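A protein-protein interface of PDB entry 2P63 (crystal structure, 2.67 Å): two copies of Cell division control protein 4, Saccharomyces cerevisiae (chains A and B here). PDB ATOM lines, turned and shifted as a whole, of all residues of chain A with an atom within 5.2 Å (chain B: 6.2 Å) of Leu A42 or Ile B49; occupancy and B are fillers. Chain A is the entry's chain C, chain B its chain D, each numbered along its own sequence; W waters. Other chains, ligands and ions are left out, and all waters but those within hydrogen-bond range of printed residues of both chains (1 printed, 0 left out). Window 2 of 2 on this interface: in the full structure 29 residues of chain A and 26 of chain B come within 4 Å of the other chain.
The side-chain hydroxyl (OG) of Ser A43 lies within hydrogen-bond range of the backbone carbonyl oxygen (O) of Ser A40.
Among the printed residues, pairs that only touch across the chains: Arg A39 with Leu B53 (3.1 Å), Ile A49 with Leu B45 (3.3 Å), Ile A49 with Ile B49 (3.3 Å), Leu A42 with Leu B53 (3.4 Å), Leu A42 with Ile B49 (3.5 Å), Ser A43 with Leu B53 (3.6 Å) and Leu A45 with Ile B49 (3.8 Å).
Of the printed residues of chain B, Arg A39 touches Leu B53 (3.1 Å).
Leu A42 touches two residues of chain B.
Of the printed residues of chain B, Ser A43 touches Leu B53 (3.6 Å).
Of the printed residues of chain B, Leu A45 touches Ile B49.
Of the printed residues of chain A, Leu B45 touches Ile A49 (3.3 Å).
Ile B49 touches just these residues of chain A: Leu A42 (3.5 Å), Leu A45 (3.8 Å) and Ile A49 (3.3 Å).
The nearest residue of chain A that does not touch Ile B49 is Gly A46 (4.6 Å).
Of the 12 printed residues of chain A, 5 touch a printed residue of chain B.
Hydrophobic or aromatic side chains of chain A within 4 Å of the printed part of chain B: Leu A42, Leu A45 and Ile A49.
Of the 11 printed residues of chain B, 3 touch a printed residue of chain A.
Hydrophobic or aromatic side chains of chain B that line the printed part of chain A: Leu B45, Ile B49 and Leu B53.
Along chain B the printed residues that touch a printed residue of chain A span positions 45 to 53.
Among the printed residues, 7 pairs touch across the chains.
Among the printed residues, no Asp or Glu carboxylate lies within 4 Å of a Lys or Arg side-chain nitrogen of the other chain.
Leu A45 touches Ile B49, and with the chains exchanged Ile A49 touches Leu B45.
Ile B49 touches its own counterpart, Ile A49.
Water W1 bridges O of Val A34 (2.6 Å) and OD1 of Asn B52 (3.1 Å).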
ATOM      1  N   VAL A  34      -5.943  -5.407  -3.076  1.00  0.00           N
ATOM      2  CA  VAL A  34      -6.736  -4.194  -3.199  1.00  0.00           C
ATOM      3  C   VAL A  34      -7.096  -3.866  -4.640  1.00  0.00           C
ATOM      4  O   VAL A  34      -8.263  -3.700  -4.997  1.00  0.00           O
ATOM      5  CB  VAL A  34      -5.951  -3.009  -2.591  1.00  0.00           C
ATOM      6  CG1 VAL A  34      -6.675  -1.695  -2.817  1.00  0.00           C
ATOM      7  CG2 VAL A  34      -5.714  -3.257  -1.108  1.00  0.00           C
ATOM      8  N   MET A  37      -9.890  -5.922  -6.243  1.00  0.00           N
ATOM      9  CA  MET A  37     -11.105  -6.096  -5.451  1.00  0.00           C
ATOM     10  C   MET A  37     -12.286  -5.381  -6.093  1.00  0.00           C
ATOM     11  O   MET A  37     -12.163  -4.239  -6.533  1.00  0.00           O
ATOM     12  CB  MET A  37     -10.922  -5.548  -4.035  1.00  0.00           C
ATOM     13  CG  MET A  37     -10.247  -6.569  -3.113  1.00  0.00           C
ATOM     14  SD  MET A  37     -10.101  -5.876  -1.293  1.00  0.00           S
ATOM     15  CE  MET A  37      -8.706  -7.178  -0.902  1.00  0.00           C
ATOM     16  N   ASP A  38     -13.446  -6.035  -6.133  1.00  0.00           N
ATOM     17  CA  ASP A  38     -14.640  -5.325  -6.594  1.00  0.00           C
ATOM     18  C   ASP A  38     -15.238  -4.513  -5.451  1.00  0.00           C
ATOM     19  O   ASP A  38     -14.745  -4.566  -4.323  1.00  0.00           O
ATOM     20  CB  ASP A  38     -15.682  -6.286  -7.151  1.00  0.00           C
ATOM     21  CG  ASP A  38     -16.124  -7.349  -6.167  1.00  0.00           C
ATOM     22  OD1 ASP A  38     -16.257  -8.516  -6.600  1.00  0.00           O
ATOM     23  OD2 ASP A  38     -16.344  -7.037  -4.980  1.00  0.00           O
ATOM     24  N   ARG A  39     -16.306  -3.782  -5.738  1.00  0.00           N
ATOM     25  CA  ARG A  39     -16.959  -2.946  -4.741  1.00  0.00           C
ATOM     26  C   ARG A  39     -17.287  -3.751  -3.486  1.00  0.00           C
ATOM     27  O   ARG A  39     -17.251  -3.224  -2.376  1.00  0.00           O
ATOM     28  CB  ARG A  39     -18.240  -2.330  -5.302  1.00  0.00           C
ATOM     29  CG  ARG A  39     -18.070  -1.059  -6.111  1.00  0.00           C
ATOM     30  CD  ARG A  39     -19.420  -0.444  -6.451  1.00  0.00           C
ATOM     31  NE  ARG A  39     -19.639   0.831  -5.771  1.00  0.00           N
ATOM     32  CZ  ARG A  39     -19.687   0.962  -4.452  1.00  0.00           C
ATOM     33  NH1 ARG A  39     -19.535  -0.106  -3.676  1.00  0.00           N
ATOM     34  NH2 ARG A  39     -19.887   2.147  -3.892  1.00  0.00           N
ATOM     35  N   SER A  40     -17.610  -5.022  -3.694  1.00  0.00           N
ATOM     36  CA  SER A  40     -18.041  -5.923  -2.636  1.00  0.00           C
ATOM     37  C   SER A  40     -16.922  -6.183  -1.640  1.00  0.00           C
ATOM     38  O   SER A  40     -17.083  -5.965  -0.439  1.00  0.00           O
ATOM     39  CB  SER A  40     -18.531  -7.241  -3.245  1.00  0.00           C
ATOM     40  OG  SER A  40     -19.021  -8.102  -2.235  1.00  0.00           O
ATOM     41  N   GLU A  41     -15.784  -6.650  -2.152  1.00  0.00           N
ATOM     42  CA  GLU A  41     -14.669  -6.975  -1.267  1.00  0.00           C
ATOM     43  C   GLU A  41     -14.088  -5.704  -0.659  1.00  0.00           C
ATOM     44  O   GLU A  41     -13.618  -5.710   0.477  1.00  0.00           O
ATOM     45  CB  GLU A  41     -13.581  -7.745  -2.008  1.00  0.00           C
ATOM     46  CG  GLU A  41     -14.087  -8.860  -2.908  1.00  0.00           C
ATOM     47  CD  GLU A  41     -13.332  -8.903  -4.224  1.00  0.00           C
ATOM     48  OE1 GLU A  41     -12.083  -8.909  -4.194  1.00  0.00           O
ATOM     49  OE2 GLU A  41     -13.983  -8.924  -5.289  1.00  0.00           O
ATOM     50  N   LEU A  42     -14.128  -4.628  -1.437  1.00  0.00           N
ATOM     51  CA  LEU A  42     -13.631  -3.339  -0.953  1.00  0.00           C
ATOM     52  C   LEU A  42     -14.372  -3.019   0.346  1.00  0.00           C
ATOM     53  O   LEU A  42     -13.768  -2.822   1.399  1.00  0.00           O
ATOM     54  CB  LEU A  42     -13.850  -2.247  -1.975  1.00  0.00           C
ATOM     55  CG  LEU A  42     -12.758  -1.502  -2.719  1.00  0.00           C
ATOM     56  CD1 LEU A  42     -11.383  -2.134  -2.597  1.00  0.00           C
ATOM     57  CD2 LEU A  42     -13.157  -1.406  -4.193  1.00  0.00           C
ATOM     58  N   SER A  43     -15.697  -2.988   0.215  1.00  0.00           N
ATOM     59  CA  SER A  43     -16.585  -2.685   1.329  1.00  0.00           C
ATOM     60  C   SER A  43     -16.366  -3.669   2.472  1.00  0.00           C
ATOM     61  O   SER A  43     -16.463  -3.339   3.649  1.00  0.00           O
ATOM     62  CB  SER A  43     -18.048  -2.729   0.889  1.00  0.00           C
ATOM     63  OG  SER A  43     -18.702  -3.839   1.488  1.00  0.00           O
ATOM     64  N   ASP A  44     -16.056  -4.911   2.102  1.00  0.00           N
ATOM     65  CA  ASP A  44     -15.735  -5.891   3.132  1.00  0.00           C
ATOM     66  C   ASP A  44     -14.598  -5.393   4.011  1.00  0.00           C
ATOM     67  O   ASP A  44     -14.773  -5.160   5.206  1.00  0.00           O
ATOM     68  CB  ASP A  44     -15.360  -7.229   2.496  1.00  0.00           C
ATOM     69  CG  ASP A  44     -16.576  -8.124   2.323  1.00  0.00           C
ATOM     70  OD1 ASP A  44     -17.636  -7.777   2.888  1.00  0.00           O
ATOM     71  OD2 ASP A  44     -16.444  -9.153   1.630  1.00  0.00           O
ATOM     72  N   LEU A  45     -13.431  -5.240   3.400  1.00  0.00           N
ATOM     73  CA  LEU A  45     -12.224  -4.872   4.135  1.00  0.00           C
ATOM     74  C   LEU A  45     -12.339  -3.562   4.892  1.00  0.00           C
ATOM     75  O   LEU A  45     -11.697  -3.358   5.927  1.00  0.00           O
ATOM     76  CB  LEU A  45     -11.040  -4.812   3.155  1.00  0.00           C
ATOM     77  CG  LEU A  45      -9.791  -4.133   3.724  1.00  0.00           C
ATOM     78  CD1 LEU A  45      -9.308  -4.860   4.972  1.00  0.00           C
ATOM     79  CD2 LEU A  45      -8.685  -4.058   2.686  1.00  0.00           C
ATOM     80  N   GLY A  46     -13.153  -2.625   4.402  1.00  0.00           N
ATOM     81  CA  GLY A  46     -13.312  -1.371   5.137  1.00  0.00           C
ATOM     82  C   GLY A  46     -13.976  -1.638   6.478  1.00  0.00           C
ATOM     83  O   GLY A  46     -13.427  -1.324   7.532  1.00  0.00           O
ATOM     84  N   ILE A  49     -11.595  -3.175   8.522  1.00  0.00           N
ATOM     85  CA  ILE A  49     -10.595  -2.245   9.062  1.00  0.00           C
ATOM     86  C   ILE A  49     -11.256  -1.438  10.176  1.00  0.00           C
ATOM     87  O   ILE A  49     -10.677  -1.259  11.245  1.00  0.00           O
ATOM     88  CB  ILE A  49     -10.018  -1.307   7.994  1.00  0.00           C
ATOM     89  CG1 ILE A  49      -8.824  -1.887   7.228  1.00  0.00           C
ATOM     90  CG2 ILE A  49      -9.656   0.042   8.599  1.00  0.00           C
ATOM     91  CD1 ILE A  49      -8.916  -1.674   5.735  1.00  0.00           C
ATOM     92  N   ASP B  44      -4.547   4.752   7.043  1.00  0.00           N
ATOM     93  CA  ASP B  44      -4.066   5.034   5.696  1.00  0.00           C
ATOM     94  C   ASP B  44      -4.852   4.221   4.671  1.00  0.00           C
ATOM     95  O   ASP B  44      -5.557   4.790   3.839  1.00  0.00           O
ATOM     96  CB  ASP B  44      -2.575   4.728   5.555  1.00  0.00           C
ATOM     97  CG  ASP B  44      -1.688   5.760   6.222  1.00  0.00           C
ATOM     98  OD1 ASP B  44      -2.168   6.883   6.494  1.00  0.00           O
ATOM     99  OD2 ASP B  44      -0.504   5.445   6.474  1.00  0.00           O
ATOM    100  N   LEU B  45      -4.717   2.903   4.765  1.00  0.00           N
ATOM    101  CA  LEU B  45      -5.421   1.995   3.860  1.00  0.00           C
ATOM    102  C   LEU B  45      -6.924   2.111   4.068  1.00  0.00           C
ATOM    103  O   LEU B  45      -7.722   1.896   3.154  1.00  0.00           O
ATOM    104  CB  LEU B  45      -4.921   0.572   4.068  1.00  0.00           C
ATOM    105  CG  LEU B  45      -5.915  -0.569   3.878  1.00  0.00           C
ATOM    106  CD1 LEU B  45      -5.785  -1.185   2.495  1.00  0.00           C
ATOM    107  CD2 LEU B  45      -5.708  -1.615   4.967  1.00  0.00           C
ATOM    108  N   GLY B  46      -7.330   2.476   5.285  1.00  0.00           N
ATOM    109  CA  GLY B  46      -8.738   2.755   5.529  1.00  0.00           C
ATOM    110  C   GLY B  46      -9.261   3.786   4.532  1.00  0.00           C
ATOM    111  O   GLY B  46     -10.088   3.442   3.686  1.00  0.00           O
ATOM    112  N   THR B  47      -8.772   5.013   4.640  1.00  0.00           N
ATOM    113  CA  THR B  47      -9.075   6.127   3.762  1.00  0.00           C
ATOM    114  C   THR B  47      -9.113   5.732   2.287  1.00  0.00           C
ATOM    115  O   THR B  47     -10.067   6.020   1.569  1.00  0.00           O
ATOM    116  CB  THR B  47      -8.021   7.253   3.871  1.00  0.00           C
ATOM    117  OG1 THR B  47      -7.664   7.477   5.236  1.00  0.00           O
ATOM    118  CG2 THR B  47      -8.607   8.551   3.334  1.00  0.00           C
ATOM    119  N   LEU B  48      -8.041   5.080   1.849  1.00  0.00           N
ATOM    120  CA  LEU B  48      -7.912   4.634   0.466  1.00  0.00           C
ATOM    121  C   LEU B  48      -9.110   3.811   0.021  1.00  0.00           C
ATOM    122  O   LEU B  48      -9.635   4.040  -1.072  1.00  0.00           O
ATOM    123  CB  LEU B  48      -6.622   3.830   0.299  1.00  0.00           C
ATOM    124  CG  LEU B  48      -6.492   2.885  -0.891  1.00  0.00           C
ATOM    125  CD1 LEU B  48      -6.175   3.654  -2.165  1.00  0.00           C
ATOM    126  CD2 LEU B  48      -5.417   1.836  -0.625  1.00  0.00           C
ATOM    127  N   ILE B  49      -9.558   2.850   0.837  1.00  0.00           N
ATOM    128  CA  ILE B  49     -10.684   2.034   0.370  1.00  0.00           C
ATOM    129  C   ILE B  49     -11.897   2.931   0.142  1.00  0.00           C
ATOM    130  O   ILE B  49     -12.615   2.787  -0.846  1.00  0.00           O
ATOM    131  CB  ILE B  49     -11.064   0.907   1.341  1.00  0.00           C
ATOM    132  CG1 ILE B  49     -10.061  -0.245   1.392  1.00  0.00           C
ATOM    133  CG2 ILE B  49     -12.462   0.391   1.028  1.00  0.00           C
ATOM    134  CD1 ILE B  49      -9.388  -0.363   2.744  1.00  0.00           C
ATOM    135  N   LYS B  50     -12.084   3.848   1.082  1.00  0.00           N
ATOM    136  CA  LYS B  50     -13.175   4.816   0.975  1.00  0.00           C
ATOM    137  C   LYS B  50     -13.181   5.484  -0.399  1.00  0.00           C
ATOM    138  O   LYS B  50     -14.131   5.302  -1.161  1.00  0.00           O
ATOM    139  CB  LYS B  50     -13.067   5.877   2.075  1.00  0.00           C
ATOM    140  CG  LYS B  50     -14.340   6.680   2.276  1.00  0.00           C
ATOM    141  CD  LYS B  50     -14.242   7.614   3.470  1.00  0.00           C
ATOM    142  CE  LYS B  50     -15.624   8.080   3.910  1.00  0.00           C
ATOM    143  NZ  LYS B  50     -15.561   9.162   4.932  1.00  0.00           N
ATOM    144  N   ASP B  51     -12.111   6.220  -0.675  1.00  0.00           N
ATOM    145  CA  ASP B  51     -11.889   6.869  -1.957  1.00  0.00           C
ATOM    146  C   ASP B  51     -12.213   5.912  -3.100  1.00  0.00           C
ATOM    147  O   ASP B  51     -13.072   6.195  -3.929  1.00  0.00           O
ATOM    148  CB  ASP B  51     -10.442   7.344  -2.085  1.00  0.00           C
ATOM    149  CG  ASP B  51     -10.093   8.465  -1.130  1.00  0.00           C
ATOM    150  OD1 ASP B  51     -10.871   9.438  -1.040  1.00  0.00           O
ATOM    151  OD2 ASP B  51      -9.037   8.368  -0.468  1.00  0.00           O
ATOM    152  N   ASN B  52     -11.511   4.786  -3.100  1.00  0.00           N
ATOM    153  CA  ASN B  52     -11.722   3.711  -4.057  1.00  0.00           C
ATOM    154  C   ASN B  52     -13.214   3.414  -4.200  1.00  0.00           C
ATOM    155  O   ASN B  52     -13.696   3.152  -5.301  1.00  0.00           O
ATOM    156  CB  ASN B  52     -10.987   2.443  -3.628  1.00  0.00           C
ATOM    157  CG  ASN B  52      -9.639   2.226  -4.278  1.00  0.00           C
ATOM    158  OD1 ASN B  52      -9.151   1.096  -4.387  1.00  0.00           O
ATOM    159  ND2 ASN B  52      -9.000   3.302  -4.720  1.00  0.00           N
ATOM    160  N   LEU B  53     -13.930   3.453  -3.079  1.00  0.00           N
ATOM    161  CA  LEU B  53     -15.360   3.158  -3.077  1.00  0.00           C
ATOM    162  C   LEU B  53     -16.167   4.372  -3.529  1.00  0.00           C
ATOM    163  O   LEU B  53     -16.985   4.277  -4.447  1.00  0.00           O
ATOM    164  CB  LEU B  53     -15.797   2.713  -1.687  1.00  0.00           C
ATOM    165  CG  LEU B  53     -16.316   1.301  -1.451  1.00  0.00           C
ATOM    166  CD1 LEU B  53     -16.604   0.559  -2.746  1.00  0.00           C
ATOM    167  CD2 LEU B  53     -15.325   0.507  -0.605  1.00  0.00           C
ATOM    168  N   LYS B  54     -15.931   5.507  -2.884  1.00  0.00           N
ATOM    169  CA  LYS B  54     -16.640   6.754  -3.099  1.00  0.00           C
ATOM    170  C   LYS B  54     -16.838   7.112  -4.568  1.00  0.00           C
ATOM    171  O   LYS B  54     -17.839   7.753  -4.893  1.00  0.00           O
ATOM    172  CB  LYS B  54     -15.897   7.925  -2.437  1.00  0.00           C
ATOM    173  CG  LYS B  54     -15.593   9.043  -3.427  1.00  0.00           C
ATOM    174  CD  LYS B  54     -14.591  10.032  -2.857  1.00  0.00           C
ATOM    175  CE  LYS B  54     -15.111  11.459  -2.921  1.00  0.00           C
ATOM    176  NZ  LYS B  54     -14.437  12.335  -1.921  1.00  0.00           N
HETATM  177  O   HOH W   1      -9.413  -1.572  -5.907  1.00  0.00           O
